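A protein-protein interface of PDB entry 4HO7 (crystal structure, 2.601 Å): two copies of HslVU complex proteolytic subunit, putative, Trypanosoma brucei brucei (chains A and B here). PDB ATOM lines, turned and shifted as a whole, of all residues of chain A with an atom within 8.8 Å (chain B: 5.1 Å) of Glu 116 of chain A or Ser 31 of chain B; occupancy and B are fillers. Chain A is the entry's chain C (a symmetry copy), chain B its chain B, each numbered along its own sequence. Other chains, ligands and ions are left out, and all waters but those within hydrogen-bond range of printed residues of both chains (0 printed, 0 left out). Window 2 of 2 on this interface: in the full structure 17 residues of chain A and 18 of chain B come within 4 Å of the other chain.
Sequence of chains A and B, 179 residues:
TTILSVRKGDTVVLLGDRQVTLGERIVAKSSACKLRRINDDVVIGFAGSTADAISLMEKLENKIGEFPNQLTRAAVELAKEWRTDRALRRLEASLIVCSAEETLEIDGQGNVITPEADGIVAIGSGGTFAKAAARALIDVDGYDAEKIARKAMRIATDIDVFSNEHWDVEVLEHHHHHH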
ATOM      1  N   ARG A   7       6.499  21.349  -0.626  1.00  0.00           N
ATOM      2  CA  ARG A   7       6.053  20.355  -1.585  1.00  0.00           C
ATOM      3  C   ARG A   7       5.318  19.305  -0.813  1.00  0.00           C
ATOM      4  O   ARG A   7       5.873  18.658   0.088  1.00  0.00           O
ATOM      5  CB  ARG A   7       7.259  19.738  -2.294  1.00  0.00           C
ATOM      6  CG  ARG A   7       6.935  18.490  -3.147  1.00  0.00           C
ATOM      7  CD  ARG A   7       8.148  18.015  -3.927  1.00  0.00           C
ATOM      8  NE  ARG A   7       8.383  18.856  -5.109  1.00  0.00           N
ATOM      9  CZ  ARG A   7       9.317  19.813  -5.211  1.00  0.00           C
ATOM     10  NH1 ARG A   7      10.170  20.081  -4.197  1.00  0.00           N
ATOM     11  NH2 ARG A   7       9.410  20.509  -6.342  1.00  0.00           N
ATOM     12  N   THR A 103      13.584  21.010  -5.535  1.00  0.00           N
ATOM     13  CA  THR A 103      13.686  22.334  -4.906  1.00  0.00           C
ATOM     14  C   THR A 103      15.058  22.497  -4.303  1.00  0.00           C
ATOM     15  O   THR A 103      15.483  21.627  -3.560  1.00  0.00           O
ATOM     16  CB  THR A 103      12.680  22.555  -3.757  1.00  0.00           C
ATOM     17  OG1 THR A 103      11.349  22.265  -4.193  1.00  0.00           O
ATOM     18  CG2 THR A 103      12.714  23.984  -3.288  1.00  0.00           C
ATOM     19  N   VAL A 112      24.402  24.172  -0.947  1.00  0.00           N
ATOM     20  CA  VAL A 112      23.337  23.833  -1.875  1.00  0.00           C
ATOM     21  C   VAL A 112      22.527  22.751  -1.170  1.00  0.00           C
ATOM     22  O   VAL A 112      23.003  21.648  -0.980  1.00  0.00           O
ATOM     23  CB  VAL A 112      23.883  23.304  -3.209  1.00  0.00           C
ATOM     24  CG1 VAL A 112      22.733  22.909  -4.136  1.00  0.00           C
ATOM     25  CG2 VAL A 112      24.738  24.375  -3.860  1.00  0.00           C
ATOM     26  N   ILE A 113      21.309  23.110  -0.793  1.00  0.00           N
ATOM     27  CA  ILE A 113      20.524  22.365   0.113  1.00  0.00           C
ATOM     28  C   ILE A 113      19.250  21.963  -0.559  1.00  0.00           C
ATOM     29  O   ILE A 113      18.540  22.768  -1.109  1.00  0.00           O
ATOM     30  CB  ILE A 113      20.210  23.264   1.281  1.00  0.00           C
ATOM     31  CG1 ILE A 113      21.468  23.361   2.143  1.00  0.00           C
ATOM     32  CG2 ILE A 113      19.035  22.780   2.121  1.00  0.00           C
ATOM     33  CD1 ILE A 113      21.450  24.577   3.021  1.00  0.00           C
ATOM     34  N   THR A 114      18.976  20.684  -0.485  1.00  0.00           N
ATOM     35  CA  THR A 114      17.695  20.152  -0.886  1.00  0.00           C
ATOM     36  C   THR A 114      16.926  19.795   0.371  1.00  0.00           C
ATOM     37  O   THR A 114      17.535  19.512   1.399  1.00  0.00           O
ATOM     38  CB  THR A 114      17.854  18.843  -1.674  1.00  0.00           C
ATOM     39  OG1 THR A 114      18.666  17.948  -0.908  1.00  0.00           O
ATOM     40  CG2 THR A 114      18.492  19.120  -2.999  1.00  0.00           C
ATOM     41  N   PRO A 115      15.581  19.735   0.262  1.00  0.00           N
ATOM     42  CA  PRO A 115      14.746  19.404   1.407  1.00  0.00           C
ATOM     43  C   PRO A 115      15.027  18.044   1.931  1.00  0.00           C
ATOM     44  O   PRO A 115      15.560  17.201   1.230  1.00  0.00           O
ATOM     45  CB  PRO A 115      13.325  19.460   0.847  1.00  0.00           C
ATOM     46  CG  PRO A 115      13.464  19.402  -0.636  1.00  0.00           C
ATOM     47  CD  PRO A 115      14.781  20.012  -0.952  1.00  0.00           C
ATOM     48  N   GLU A 116      14.651  17.832   3.175  1.00  0.00           N
ATOM     49  CA  GLU A 116      14.532  16.479   3.706  1.00  0.00           C
ATOM     50  C   GLU A 116      13.281  15.867   3.070  1.00  0.00           C
ATOM     51  O   GLU A 116      12.693  16.451   2.178  1.00  0.00           O
ATOM     52  CB  GLU A 116      14.400  16.492   5.236  1.00  0.00           C
ATOM     53  CG  GLU A 116      15.338  17.440   5.984  1.00  0.00           C
ATOM     54  CD  GLU A 116      16.800  17.038   5.994  1.00  0.00           C
ATOM     55  OE1 GLU A 116      17.144  15.889   5.631  1.00  0.00           O
ATOM     56  OE2 GLU A 116      17.619  17.908   6.394  1.00  0.00           O
ATOM     57  N   ALA A 117      12.873  14.692   3.510  1.00  0.00           N
ATOM     58  CA  ALA A 117      11.686  14.048   2.930  1.00  0.00           C
ATOM     59  C   ALA A 117      10.435  14.934   2.998  1.00  0.00           C
ATOM     60  O   ALA A 117       9.557  14.805   2.178  1.00  0.00           O
ATOM     61  CB  ALA A 117      11.425  12.736   3.635  1.00  0.00           C
ATOM     62  N   ASP A 118      10.377  15.864   3.951  1.00  0.00           N
ATOM     63  CA  ASP A 118       9.164  16.645   4.164  1.00  0.00           C
ATOM     64  C   ASP A 118       8.897  17.706   3.111  1.00  0.00           C
ATOM     65  O   ASP A 118       7.834  18.360   3.131  1.00  0.00           O
ATOM     66  CB  ASP A 118       9.193  17.289   5.545  1.00  0.00           C
ATOM     67  CG  ASP A 118      10.371  18.223   5.743  1.00  0.00           C
ATOM     68  OD1 ASP A 118      10.849  18.854   4.767  1.00  0.00           O
ATOM     69  OD2 ASP A 118      10.786  18.364   6.910  1.00  0.00           O
ATOM     70  N   GLY A 119       9.872  17.929   2.238  1.00  0.00           N
ATOM     71  CA  GLY A 119       9.673  18.814   1.092  1.00  0.00           C
ATOM     72  C   GLY A 119       9.703  20.274   1.405  1.00  0.00           C
ATOM     73  O   GLY A 119       9.277  21.096   0.603  1.00  0.00           O
ATOM     74  N   ILE A 120      10.251  20.601   2.549  1.00  0.00           N
ATOM     75  CA  ILE A 120      10.305  21.992   3.006  1.00  0.00           C
ATOM     76  C   ILE A 120      11.689  22.668   2.951  1.00  0.00           C
ATOM     77  O   ILE A 120      12.714  22.124   3.388  1.00  0.00           O
ATOM     78  CB  ILE A 120       9.794  22.059   4.434  1.00  0.00           C
ATOM     79  CG1 ILE A 120       8.333  21.582   4.452  1.00  0.00           C
ATOM     80  CG2 ILE A 120       9.886  23.470   4.967  1.00  0.00           C
ATOM     81  CD1 ILE A 120       7.878  21.173   5.833  1.00  0.00           C
ATOM     82  N   VAL A 121      11.689  23.861   2.380  1.00  0.00           N
ATOM     83  CA  VAL A 121      12.896  24.666   2.195  1.00  0.00           C
ATOM     84  C   VAL A 121      12.510  26.103   2.503  1.00  0.00           C
ATOM     85  O   VAL A 121      11.428  26.576   2.082  1.00  0.00           O
ATOM     86  CB  VAL A 121      13.413  24.520   0.736  1.00  0.00           C
ATOM     87  CG1 VAL A 121      14.458  25.540   0.363  1.00  0.00           C
ATOM     88  CG2 VAL A 121      14.029  23.149   0.547  1.00  0.00           C
ATOM     89  N   LYS A 131      10.026  27.355   8.429  1.00  0.00           N
ATOM     90  CA  LYS A 131      10.279  25.938   8.255  1.00  0.00           C
ATOM     91  C   LYS A 131       9.677  25.179   9.429  1.00  0.00           C
ATOM     92  O   LYS A 131       9.080  24.104   9.292  1.00  0.00           O
ATOM     93  CB  LYS A 131      11.769  25.671   8.131  1.00  0.00           C
ATOM     94  CG  LYS A 131      12.129  24.210   8.013  1.00  0.00           C
ATOM     95  CD  LYS A 131      13.632  23.960   8.174  1.00  0.00           C
ATOM     96  CE  LYS A 131      14.409  24.142   6.881  1.00  0.00           C
ATOM     97  NZ  LYS A 131      15.837  24.124   7.258  1.00  0.00           N
ATOM     98  N   ARG A 135       6.775  22.365   9.162  1.00  0.00           N
ATOM     99  CA  ARG A 135       7.017  20.998   9.573  1.00  0.00           C
ATOM    100  C   ARG A 135       5.998  20.476  10.560  1.00  0.00           C
ATOM    101  O   ARG A 135       5.789  19.236  10.667  1.00  0.00           O
ATOM    102  CB  ARG A 135       8.369  20.850  10.181  1.00  0.00           C
ATOM    103  CG  ARG A 135       9.444  20.799   9.143  1.00  0.00           C
ATOM    104  CD  ARG A 135      10.820  20.621   9.767  1.00  0.00           C
ATOM    105  NE  ARG A 135      11.856  20.446   8.738  1.00  0.00           N
ATOM    106  CZ  ARG A 135      13.160  20.469   8.968  1.00  0.00           C
ATOM    107  NH1 ARG A 135      13.607  20.689  10.217  1.00  0.00           N
ATOM    108  NH2 ARG A 135      14.024  20.264   7.969  1.00  0.00           N
ATOM    109  N   ILE A 138       3.064  19.281   8.255  1.00  0.00           N
ATOM    110  CA  ILE A 138       3.308  18.628   6.972  1.00  0.00           C
ATOM    111  C   ILE A 138       2.554  17.296   6.864  1.00  0.00           C
ATOM    112  O   ILE A 138       2.125  16.873   5.789  1.00  0.00           O
ATOM    113  CB  ILE A 138       4.818  18.419   6.766  1.00  0.00           C
ATOM    114  CG1 ILE A 138       5.118  18.044   5.312  1.00  0.00           C
ATOM    115  CG2 ILE A 138       5.374  17.381   7.759  1.00  0.00           C
ATOM    116  CD1 ILE A 138       4.842  19.136   4.300  1.00  0.00           C
ATOM    117  N   ARG B  18      26.390  14.094   8.156  1.00  0.00           N
ATOM    118  CA  ARG B  18      25.556  14.651   7.091  1.00  0.00           C
ATOM    119  C   ARG B  18      24.883  15.963   7.450  1.00  0.00           C
ATOM    120  O   ARG B  18      23.964  16.384   6.760  1.00  0.00           O
ATOM    121  CB  ARG B  18      24.534  13.586   6.625  1.00  0.00           C
ATOM    122  CG  ARG B  18      25.228  12.323   6.092  1.00  0.00           C
ATOM    123  CD  ARG B  18      24.394  11.039   6.053  1.00  0.00           C
ATOM    124  NE  ARG B  18      24.038  10.723   4.672  1.00  0.00           N
ATOM    125  CZ  ARG B  18      22.831  10.870   4.167  1.00  0.00           C
ATOM    126  NH1 ARG B  18      21.825  11.260   4.935  1.00  0.00           N
ATOM    127  NH2 ARG B  18      22.637  10.597   2.892  1.00  0.00           N
ATOM    128  N   ALA B  28      20.463  23.155   8.796  1.00  0.00           N
ATOM    129  CA  ALA B  28      19.668  23.401   7.603  1.00  0.00           C
ATOM    130  C   ALA B  28      19.426  22.127   6.809  1.00  0.00           C
ATOM    131  O   ALA B  28      18.533  22.085   6.026  1.00  0.00           O
ATOM    132  CB  ALA B  28      20.345  24.473   6.728  1.00  0.00           C
ATOM    133  N   LYS B  29      20.281  21.124   6.955  1.00  0.00           N
ATOM    134  CA  LYS B  29      20.075  19.854   6.286  1.00  0.00           C
ATOM    135  C   LYS B  29      20.747  18.810   7.146  1.00  0.00           C
ATOM    136  O   LYS B  29      21.884  19.018   7.634  1.00  0.00           O
ATOM    137  CB  LYS B  29      20.676  19.861   4.874  1.00  0.00           C
ATOM    138  CG  LYS B  29      20.244  18.708   3.975  1.00  0.00           C
ATOM    139  CD  LYS B  29      20.799  18.846   2.544  1.00  0.00           C
ATOM    140  CE  LYS B  29      20.463  17.670   1.633  1.00  0.00           C
ATOM    141  NZ  LYS B  29      18.999  17.406   1.647  1.00  0.00           N
ATOM    142  N   SER B  30      20.055  17.695   7.340  1.00  0.00           N
ATOM    143  CA  SER B  30      20.621  16.617   8.139  1.00  0.00           C
ATOM    144  C   SER B  30      20.982  15.384   7.289  1.00  0.00           C
ATOM    145  O   SER B  30      21.311  14.338   7.825  1.00  0.00           O
ATOM    146  CB  SER B  30      19.673  16.257   9.269  1.00  0.00           C
ATOM    147  OG  SER B  30      18.410  16.000   8.754  1.00  0.00           O
ATOM    148  N   SER B  31      21.006  15.549   5.967  1.00  0.00           N
ATOM    149  CA  SER B  31      21.146  14.433   5.022  1.00  0.00           C
ATOM    150  C   SER B  31      22.068  14.753   3.821  1.00  0.00           C
ATOM    151  O   SER B  31      21.884  14.261   2.715  1.00  0.00           O
ATOM    152  CB  SER B  31      19.761  14.085   4.520  1.00  0.00           C
ATOM    153  OG  SER B  31      19.214  15.224   3.885  1.00  0.00           O
ATOM    154  N   ALA B  32      23.056  15.602   4.059  1.00  0.00           N
ATOM    155  CA  ALA B  32      24.020  16.008   3.034  1.00  0.00           C
ATOM    156  C   ALA B  32      25.244  15.097   3.035  1.00  0.00           C
ATOM    157  O   ALA B  32      25.853  14.882   4.071  1.00  0.00           O
ATOM    158  CB  ALA B  32      24.462  17.431   3.297  1.00  0.00           C
ATOM    159  N   CYS B  33      25.618  14.578   1.883  1.00  0.00           N
ATOM    160  CA  CYS B  33      26.728  13.665   1.769  1.00  0.00           C
ATOM    161  C   CYS B  33      28.004  14.440   1.651  1.00  0.00           C
ATOM    162  O   CYS B  33      28.103  15.346   0.842  1.00  0.00           O
ATOM    163  CB  CYS B  33      26.556  12.802   0.508  1.00  0.00           C
ATOM    164  SG  CYS B  33      27.822  11.515   0.335  1.00  0.00           S
ATOM    165  N   ASN B 164      26.110  15.349  13.144  1.00  0.00           N
ATOM    166  CA  ASN B 164      25.002  14.450  13.476  1.00  0.00           C
ATOM    167  C   ASN B 164      25.323  12.970  13.394  1.00  0.00           C
ATOM    168  O   ASN B 164      26.454  12.577  13.116  1.00  0.00           O
ATOM    169  CB  ASN B 164      23.734  14.781  12.671  1.00  0.00           C
ATOM    170  CG  ASN B 164      23.846  14.475  11.187  1.00  0.00           C
ATOM    171  OD1 ASN B 164      24.730  13.750  10.716  1.00  0.00           O
ATOM    172  ND2 ASN B 164      22.924  15.036  10.445  1.00  0.00           N
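Ile 113 of chain A touches Ala 28 of chain B.
Lys 29 of chain B touches Glu 116 of chain A.
Lys 131 of chain A touches Ala 28 of chain B.
No position is printed for both chains.
Of the 7 pairs that touch across the chains among the printed residues, none has its exchanged pair printed and touching as well.
Of chain B, only Lys 29, Ser 30 and Ser 31 come within 4 Å of Glu 116 of chain A.
Of the printed residues of chain A, Ser 31 of chain B touches Glu 116.
Ser 30 of chain B touches just one residue of chain A: Glu 116.
No residue of chain A comes within 4 Å of Ala 32 of chain B.
Printed residues of chain B within 4 Å of Lys 131 of chain A: Ala 28 (3.6 Å).
Printed residues of chain B within 4 Å of Ile 113 of chain A: Ala 28 (3.9 Å).
Of the printed residues of chain A, Ala 28 of chain B touches Ile 113 and Lys 131.
Printed residues of chain B within 4 Å of Pro 115 of chain A: Lys 29.
Of the printed residues of chain B, Thr 114 of chain A touches Lys 29 (2.6 Å).
The nearest residue of chain B that does not touch Glu 116 of chain A is Ala 28 of chain B (4.3 Å).
Of the 15 printed residues of chain A, 5 touch a printed residue of chain B.
Hydrophobic or aromatic side chains of chain B within 4 Å of the printed part of chain A: Ala 28.
Among the printed residues, no Asp or Glu carboxylate lies within 4 Å of a Lys or Arg side-chain nitrogen of the other chain.
The side-chain carboxylate of Glu 116 of chain A sits at hydrogen-bond distance from the backbone NH of Ser 30 of chain B (2.6 Å).
NZ of Lys 29 of chain B is in hydrogen-bond range of O of Thr 114 of chain A, 2.6 Å away.
The side-chain hydroxyl (OG) of Ser 31 of chain B lies within hydrogen-bond range of the side-chain carboxylate (OE1) of Glu 116 of chain A, at 2.8 Å.
O of Pro 115 of chain A sits at hydrogen-bond distance from NZ of Lys 29 of chain B, 3.5 Å away.
O of Arg 18 of chain B lies within hydrogen-bond range of N of Ser 31 of chain B, 3.2 Å away.
The side-chain hydroxyl of Ser 31 of chain B is in hydrogen-bond range of the side-chain amino group of Lys 29 of chain B (3.1 Å).
The side-chain amide nitrogen (ND2) of Asn 164 of chain B lies within hydrogen-bond range of the backbone carbonyl oxygen (O) of Ser 30 of chain B, at 3.2 Å.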
